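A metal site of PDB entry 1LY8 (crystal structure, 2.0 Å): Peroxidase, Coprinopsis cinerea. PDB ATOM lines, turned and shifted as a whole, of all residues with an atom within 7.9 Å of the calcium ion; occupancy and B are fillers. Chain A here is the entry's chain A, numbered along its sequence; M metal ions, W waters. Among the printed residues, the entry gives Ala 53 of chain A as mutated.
The side-chain carboxylate (OD1) of Asp 56 sits close to the backbone NH (N) of Ile 79.
OD1 of Asp 76 lies close to N of Gly 73.
OD2 of Asp 56 is in hydrogen-bond range of N of Gly 77 (2.8 Å).
The side-chain hydroxyl (OG) of Ser 78 lies close to the side-chain carboxylate (OE2) of Glu 86 (2.6 Å).
The backbone NH (N) of Gly 74 is in hydrogen-bond range of the backbone carbonyl oxygen (O) of Gly 59 (3.1 Å).
Four residues have an atom within 4 Å of the calcium ion: Asp 56, Gly 74, Asp 76 and Ser 78.
The calcium ion is bound by OG of Ser 78 (2.4 Å), OD1 of Asp 56 (2.4 Å), O of Asp 56 (2.4 Å), water W1 (2.4 Å), O of Gly 74 (2.5 Å), water W2 (2.5 Å) and OD2 of Asp 76 (2.7 Å).
The calcium ion has seven donor atoms within binding distance.
Water W2 bridges OE1 of Glu 86 (2.6 Å) and O of His 55 (3.1 Å).
Water W1 bridges the backbone carbonyl oxygen (O) of Gly 59 (2.7 Å) and the backbone NH (N) of Gly 74 (3.5 Å).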
ATOM      1  N   ILE A  52     -14.214  30.634  20.832  1.00  0.00           N
ATOM      2  CA  ILE A  52     -15.665  30.674  20.980  1.00  0.00           C
ATOM      3  C   ILE A  52     -16.367  29.646  20.084  1.00  0.00           C
ATOM      4  O   ILE A  52     -17.389  29.083  20.464  1.00  0.00           O
ATOM      5  CB  ILE A  52     -16.217  32.085  20.661  1.00  0.00           C
ATOM      6  CG1 ILE A  52     -15.849  33.039  21.793  1.00  0.00           C
ATOM      7  CG2 ILE A  52     -17.729  32.040  20.466  1.00  0.00           C
ATOM      8  CD1 ILE A  52     -16.252  34.482  21.541  1.00  0.00           C
ATOM      9  N   ALA A  53     -15.817  29.415  18.890  1.00  0.00           N
ATOM     10  CA  ALA A  53     -16.395  28.457  17.968  1.00  0.00           C
ATOM     11  C   ALA A  53     -16.405  27.076  18.616  1.00  0.00           C
ATOM     12  O   ALA A  53     -17.363  26.326  18.493  1.00  0.00           O
ATOM     13  CB  ALA A  53     -15.586  28.420  16.684  1.00  0.00           C
ATOM     14  N   PHE A  54     -15.333  26.766  19.325  1.00  0.00           N
ATOM     15  CA  PHE A  54     -15.183  25.494  20.018  1.00  0.00           C
ATOM     16  C   PHE A  54     -16.133  25.411  21.206  1.00  0.00           C
ATOM     17  O   PHE A  54     -16.945  24.492  21.313  1.00  0.00           O
ATOM     18  CB  PHE A  54     -13.740  25.328  20.485  1.00  0.00           C
ATOM     19  CG  PHE A  54     -13.512  24.134  21.385  1.00  0.00           C
ATOM     20  CD1 PHE A  54     -12.660  24.244  22.485  1.00  0.00           C
ATOM     21  CD2 PHE A  54     -14.126  22.915  21.134  1.00  0.00           C
ATOM     22  CE1 PHE A  54     -12.430  23.150  23.325  1.00  0.00           C
ATOM     23  CE2 PHE A  54     -13.904  21.815  21.959  1.00  0.00           C
ATOM     24  CZ  PHE A  54     -13.053  21.925  23.059  1.00  0.00           C
ATOM     25  N   HIS A  55     -16.039  26.385  22.114  1.00  0.00           N
ATOM     26  CA  HIS A  55     -16.880  26.387  23.318  1.00  0.00           C
ATOM     27  C   HIS A  55     -18.386  26.435  23.083  1.00  0.00           C
ATOM     28  O   HIS A  55     -19.167  26.073  23.973  1.00  0.00           O
ATOM     29  CB  HIS A  55     -16.437  27.508  24.254  1.00  0.00           C
ATOM     30  CG  HIS A  55     -15.079  27.310  24.850  1.00  0.00           C
ATOM     31  ND1 HIS A  55     -14.568  28.113  25.835  1.00  0.00           N
ATOM     32  CD2 HIS A  55     -14.126  26.385  24.580  1.00  0.00           C
ATOM     33  CE1 HIS A  55     -13.346  27.698  26.155  1.00  0.00           C
ATOM     34  NE2 HIS A  55     -13.059  26.653  25.402  1.00  0.00           N
ATOM     35  N   ASP A  56     -18.824  26.868  21.908  1.00  0.00           N
ATOM     36  CA  ASP A  56     -20.258  26.882  21.641  1.00  0.00           C
ATOM     37  C   ASP A  56     -20.693  25.508  21.166  1.00  0.00           C
ATOM     38  O   ASP A  56     -21.642  24.919  21.675  1.00  0.00           O
ATOM     39  CB  ASP A  56     -20.620  27.940  20.590  1.00  0.00           C
ATOM     40  CG  ASP A  56     -22.092  27.916  20.219  1.00  0.00           C
ATOM     41  OD1 ASP A  56     -22.939  27.757  21.130  1.00  0.00           O
ATOM     42  OD2 ASP A  56     -22.428  28.067  19.016  1.00  0.00           O
ATOM     43  N   ALA A  57     -19.966  24.982  20.181  1.00  0.00           N
ATOM     44  CA  ALA A  57     -20.254  23.691  19.583  1.00  0.00           C
ATOM     45  C   ALA A  57     -20.085  22.488  20.509  1.00  0.00           C
ATOM     46  O   ALA A  57     -20.892  21.554  20.476  1.00  0.00           O
ATOM     47  CB  ALA A  57     -19.389  23.503  18.321  1.00  0.00           C
ATOM     48  N   ILE A  58     -19.040  22.509  21.331  1.00  0.00           N
ATOM     49  CA  ILE A  58     -18.752  21.398  22.234  1.00  0.00           C
ATOM     50  C   ILE A  58     -19.847  21.119  23.265  1.00  0.00           C
ATOM     51  O   ILE A  58     -19.884  20.042  23.851  1.00  0.00           O
ATOM     52  CB  ILE A  58     -17.403  21.576  22.958  1.00  0.00           C
ATOM     53  CG1 ILE A  58     -16.911  20.224  23.476  1.00  0.00           C
ATOM     54  CG2 ILE A  58     -17.545  22.553  24.103  1.00  0.00           C
ATOM     55  CD1 ILE A  58     -16.755  19.175  22.393  1.00  0.00           C
ATOM     56  N   GLY A  59     -20.741  22.080  23.485  1.00  0.00           N
ATOM     57  CA  GLY A  59     -21.822  21.868  24.418  1.00  0.00           C
ATOM     58  C   GLY A  59     -22.853  20.959  23.773  1.00  0.00           C
ATOM     59  O   GLY A  59     -23.977  21.380  23.490  1.00  0.00           O
ATOM     60  N   PHE A  60     -22.449  19.726  23.524  1.00  0.00           N
ATOM     61  CA  PHE A  60     -23.294  18.713  22.882  1.00  0.00           C
ATOM     62  C   PHE A  60     -22.906  17.378  23.515  1.00  0.00           C
ATOM     63  O   PHE A  60     -21.749  16.980  23.463  1.00  0.00           O
ATOM     64  CB  PHE A  60     -23.000  18.692  21.375  1.00  0.00           C
ATOM     65  CG  PHE A  60     -23.789  17.673  20.607  1.00  0.00           C
ATOM     66  CD1 PHE A  60     -25.141  17.856  20.369  1.00  0.00           C
ATOM     67  CD2 PHE A  60     -23.167  16.531  20.097  1.00  0.00           C
ATOM     68  CE1 PHE A  60     -25.877  16.924  19.635  1.00  0.00           C
ATOM     69  CE2 PHE A  60     -23.881  15.597  19.357  1.00  0.00           C
ATOM     70  CZ  PHE A  60     -25.243  15.789  19.129  1.00  0.00           C
ATOM     71  N   GLY A  72     -27.599  19.451  25.216  1.00  0.00           N
ATOM     72  CA  GLY A  72     -27.043  20.635  24.597  1.00  0.00           C
ATOM     73  C   GLY A  72     -27.316  20.656  23.104  1.00  0.00           C
ATOM     74  O   GLY A  72     -27.411  19.606  22.475  1.00  0.00           O
ATOM     75  N   GLY A  73     -27.423  21.857  22.533  1.00  0.00           N
ATOM     76  CA  GLY A  73     -27.701  21.975  21.114  1.00  0.00           C
ATOM     77  C   GLY A  73     -26.505  22.146  20.189  1.00  0.00           C
ATOM     78  O   GLY A  73     -26.677  22.394  18.997  1.00  0.00           O
ATOM     79  N   GLY A  74     -25.298  22.011  20.719  1.00  0.00           N
ATOM     80  CA  GLY A  74     -24.111  22.143  19.899  1.00  0.00           C
ATOM     81  C   GLY A  74     -23.870  23.558  19.382  1.00  0.00           C
ATOM     82  O   GLY A  74     -24.036  24.523  20.126  1.00  0.00           O
ATOM     83  N   ALA A  75     -23.484  23.665  18.119  1.00  0.00           N
ATOM     84  CA  ALA A  75     -23.206  24.949  17.485  1.00  0.00           C
ATOM     85  C   ALA A  75     -24.462  25.793  17.267  1.00  0.00           C
ATOM     86  O   ALA A  75     -24.690  26.316  16.177  1.00  0.00           O
ATOM     87  CB  ALA A  75     -22.499  24.731  16.154  1.00  0.00           C
ATOM     88  N   ASP A  76     -25.257  25.929  18.334  1.00  0.00           N
ATOM     89  CA  ASP A  76     -26.509  26.671  18.294  1.00  0.00           C
ATOM     90  C   ASP A  76     -26.402  28.137  18.738  1.00  0.00           C
ATOM     91  O   ASP A  76     -27.420  28.815  18.913  1.00  0.00           O
ATOM     92  CB  ASP A  76     -27.544  25.968  19.157  1.00  0.00           C
ATOM     93  CG  ASP A  76     -27.085  25.795  20.598  1.00  0.00           C
ATOM     94  OD1 ASP A  76     -27.732  25.041  21.347  1.00  0.00           O
ATOM     95  OD2 ASP A  76     -26.068  26.424  20.973  1.00  0.00           O
ATOM     96  N   GLY A  77     -25.180  28.627  18.932  1.00  0.00           N
ATOM     97  CA  GLY A  77     -24.996  30.010  19.366  1.00  0.00           C
ATOM     98  C   GLY A  77     -25.458  30.281  20.782  1.00  0.00           C
ATOM     99  O   GLY A  77     -25.629  31.434  21.188  1.00  0.00           O
ATOM    100  N   SER A  78     -25.657  29.218  21.562  1.00  0.00           N
ATOM    101  CA  SER A  78     -26.113  29.341  22.946  1.00  0.00           C
ATOM    102  C   SER A  78     -25.150  30.119  23.839  1.00  0.00           C
ATOM    103  O   SER A  78     -25.578  30.724  24.824  1.00  0.00           O
ATOM    104  CB  SER A  78     -26.332  27.961  23.551  1.00  0.00           C
ATOM    105  OG  SER A  78     -25.127  27.222  23.569  1.00  0.00           O
ATOM    106  N   ILE A  79     -23.868  30.119  23.488  1.00  0.00           N
ATOM    107  CA  ILE A  79     -22.869  30.834  24.291  1.00  0.00           C
ATOM    108  C   ILE A  79     -23.134  32.327  24.234  1.00  0.00           C
ATOM    109  O   ILE A  79     -22.718  33.079  25.120  1.00  0.00           O
ATOM    110  CB  ILE A  79     -21.421  30.517  23.814  1.00  0.00           C
ATOM    111  CG1 ILE A  79     -20.422  30.842  24.928  1.00  0.00           C
ATOM    112  CG2 ILE A  79     -21.094  31.325  22.552  1.00  0.00           C
ATOM    113  CD1 ILE A  79     -19.002  30.383  24.643  1.00  0.00           C
ATOM    114  N   ILE A  80     -23.834  32.786  23.190  1.00  0.00           N
ATOM    115  CA  ILE A  80     -24.165  34.194  23.064  1.00  0.00           C
ATOM    116  C   ILE A  80     -25.569  34.470  23.586  1.00  0.00           C
ATOM    117  O   ILE A  80     -25.754  35.319  24.457  1.00  0.00           O
ATOM    118  CB  ILE A  80     -24.085  34.676  21.600  1.00  0.00           C
ATOM    119  CG1 ILE A  80     -22.631  34.666  21.111  1.00  0.00           C
ATOM    120  CG2 ILE A  80     -24.658  36.087  21.487  1.00  0.00           C
ATOM    121  CD1 ILE A  80     -22.439  35.182  19.693  1.00  0.00           C
ATOM    122  N   HIS A  82     -27.262  32.841  25.524  1.00  0.00           N
ATOM    123  CA  HIS A  82     -27.335  32.487  26.936  1.00  0.00           C
ATOM    124  C   HIS A  82     -25.978  32.726  27.581  1.00  0.00           C
ATOM    125  O   HIS A  82     -25.522  31.937  28.402  1.00  0.00           O
ATOM    126  CB  HIS A  82     -27.739  31.014  27.070  1.00  0.00           C
ATOM    127  CG  HIS A  82     -29.044  30.681  26.427  1.00  0.00           C
ATOM    128  ND1 HIS A  82     -30.254  31.139  26.903  1.00  0.00           N
ATOM    129  CD2 HIS A  82     -29.325  29.959  25.319  1.00  0.00           C
ATOM    130  CE1 HIS A  82     -31.228  30.709  26.120  1.00  0.00           C
ATOM    131  NE2 HIS A  82     -30.691  29.990  25.147  1.00  0.00           N
ATOM    132  N   GLU A  86     -23.692  30.647  30.344  1.00  0.00           N
ATOM    133  CA  GLU A  86     -22.480  29.993  29.855  1.00  0.00           C
ATOM    134  C   GLU A  86     -21.159  30.693  30.144  1.00  0.00           C
ATOM    135  O   GLU A  86     -20.139  30.023  30.321  1.00  0.00           O
ATOM    136  CB  GLU A  86     -22.620  29.702  28.355  1.00  0.00           C
ATOM    137  CG  GLU A  86     -23.592  28.564  28.052  1.00  0.00           C
ATOM    138  CD  GLU A  86     -23.609  28.150  26.586  1.00  0.00           C
ATOM    139  OE1 GLU A  86     -22.522  28.028  25.988  1.00  0.00           O
ATOM    140  OE2 GLU A  86     -24.715  27.925  26.050  1.00  0.00           O
ATOM    141  N   GLY A 114     -25.544  31.013  15.863  1.00  0.00           N
ATOM    142  CA  GLY A 114     -24.833  29.794  15.505  1.00  0.00           C
ATOM    143  C   GLY A 114     -24.013  29.920  14.230  1.00  0.00           C
ATOM    144  O   GLY A 114     -22.827  29.585  14.200  1.00  0.00           O
ATOM    145  N   ILE A 117     -21.001  32.622  14.551  1.00  0.00           N
ATOM    146  CA  ILE A 117     -19.850  32.141  15.303  1.00  0.00           C
ATOM    147  C   ILE A 117     -18.910  31.317  14.441  1.00  0.00           C
ATOM    148  O   ILE A 117     -17.692  31.520  14.460  1.00  0.00           O
ATOM    149  CB  ILE A 117     -20.288  31.317  16.533  1.00  0.00           C
ATOM    150  CG1 ILE A 117     -20.841  32.252  17.606  1.00  0.00           C
ATOM    151  CG2 ILE A 117     -19.133  30.506  17.072  1.00  0.00           C
ATOM    152  CD1 ILE A 117     -21.440  31.542  18.821  1.00  0.00           C
ATOM    153  N   SER A 144     -32.007  28.698  20.816  1.00  0.00           N
ATOM    154  CA  SER A 144     -31.244  27.713  21.563  1.00  0.00           C
ATOM    155  C   SER A 144     -31.619  27.670  23.045  1.00  0.00           C
ATOM    156  O   SER A 144     -32.295  28.569  23.559  1.00  0.00           O
ATOM    157  CB  SER A 144     -29.751  28.003  21.451  1.00  0.00           C
ATOM    158  OG  SER A 144     -29.420  29.216  22.115  1.00  0.00           O
ATOM    159  N   GLN A 145     -31.170  26.616  23.727  1.00  0.00           N
ATOM    160  CA  GLN A 145     -31.393  26.458  25.158  1.00  0.00           C
ATOM    161  C   GLN A 145     -30.001  26.561  25.748  1.00  0.00           C
ATOM    162  O   GLN A 145     -29.017  26.224  25.074  1.00  0.00           O
ATOM    163  CB  GLN A 145     -31.964  25.065  25.480  1.00  0.00           C
ATOM    164  CG  GLN A 145     -33.387  24.840  25.011  1.00  0.00           C
ATOM    165  CD  GLN A 145     -33.867  23.426  25.278  1.00  0.00           C
ATOM    166  OE1 GLN A 145     -33.905  22.982  26.423  1.00  0.00           O
ATOM    167  NE2 GLN A 145     -34.220  22.703  24.214  1.00  0.00           N
ATOM    168  N   PRO A 146     -29.873  27.039  26.993  1.00  0.00           N
ATOM    169  CA  PRO A 146     -28.513  27.139  27.533  1.00  0.00           C
ATOM    170  C   PRO A 146     -27.817  25.784  27.562  1.00  0.00           C
ATOM    171  O   PRO A 146     -28.453  24.742  27.749  1.00  0.00           O
ATOM    172  CB  PRO A 146     -28.719  27.747  28.913  1.00  0.00           C
ATOM    173  CG  PRO A 146     -30.143  27.415  29.256  1.00  0.00           C
ATOM    174  CD  PRO A 146     -30.866  27.561  27.952  1.00  0.00           C
ATOM    175  N   SER A 147     -26.507  25.798  27.339  1.00  0.00           N
ATOM    176  CA  SER A 147     -25.726  24.572  27.346  1.00  0.00           C
ATOM    177  C   SER A 147     -25.625  23.987  28.738  1.00  0.00           C
ATOM    178  O   SER A 147     -25.524  24.719  29.718  1.00  0.00           O
ATOM    179  CB  SER A 147     -24.320  24.833  26.814  1.00  0.00           C
ATOM    180  OG  SER A 147     -23.458  23.752  27.130  1.00  0.00           O
ATOM    181  N   PRO A 148     -25.662  22.651  28.850  1.00  0.00           N
ATOM    182  CA  PRO A 148     -25.552  22.040  30.174  1.00  0.00           C
ATOM    183  C   PRO A 148     -24.133  22.351  30.640  1.00  0.00           C
ATOM    184  O   PRO A 148     -23.249  22.574  29.817  1.00  0.00           O
ATOM    185  CB  PRO A 148     -25.739  20.552  29.895  1.00  0.00           C
ATOM    186  CG  PRO A 148     -26.619  20.540  28.683  1.00  0.00           C
ATOM    187  CD  PRO A 148     -26.014  21.632  27.834  1.00  0.00           C
ATOM    188  N   LEU A 282     -22.184  20.284  14.982  1.00  0.00           N
ATOM    189  CA  LEU A 282     -22.657  19.485  16.103  1.00  0.00           C
ATOM    190  C   LEU A 282     -24.043  19.995  16.525  1.00  0.00           C
ATOM    191  O   LEU A 282     -24.223  21.194  16.770  1.00  0.00           O
ATOM    192  CB  LEU A 282     -21.689  19.586  17.284  1.00  0.00           C
ATOM    193  CG  LEU A 282     -20.385  18.785  17.164  1.00  0.00           C
ATOM    194  CD1 LEU A 282     -19.601  18.925  18.466  1.00  0.00           C
ATOM    195  CD2 LEU A 282     -20.680  17.318  16.873  1.00  0.00           C
ATOM    196  N   PHE A 284     -26.741  19.539  14.566  1.00  0.00           N
ATOM    197  CA  PHE A 284     -27.491  19.834  13.344  1.00  0.00           C
ATOM    198  C   PHE A 284     -27.267  18.781  12.276  1.00  0.00           C
ATOM    199  O   PHE A 284     -26.339  17.974  12.356  1.00  0.00           O
ATOM    200  CB  PHE A 284     -27.046  21.195  12.791  1.00  0.00           C
ATOM    201  CG  PHE A 284     -27.284  22.341  13.718  1.00  0.00           C
ATOM    202  CD1 PHE A 284     -28.503  23.008  13.743  1.00  0.00           C
ATOM    203  CD2 PHE A 284     -26.275  22.774  14.585  1.00  0.00           C
ATOM    204  CE1 PHE A 284     -28.723  24.076  14.604  1.00  0.00           C
ATOM    205  CE2 PHE A 284     -26.487  23.847  15.459  1.00  0.00           C
ATOM    206  CZ  PHE A 284     -27.716  24.499  15.468  1.00  0.00           C
HETATM  207 CA    CA M   1     -23.798  25.835  22.208  1.00  0.00          CA
HETATM  208  O   HOH W   1     -24.677  23.991  23.510  1.00  0.00           O
HETATM  209  O   HOH W   2     -22.274  26.294  24.100  1.00  0.00           O
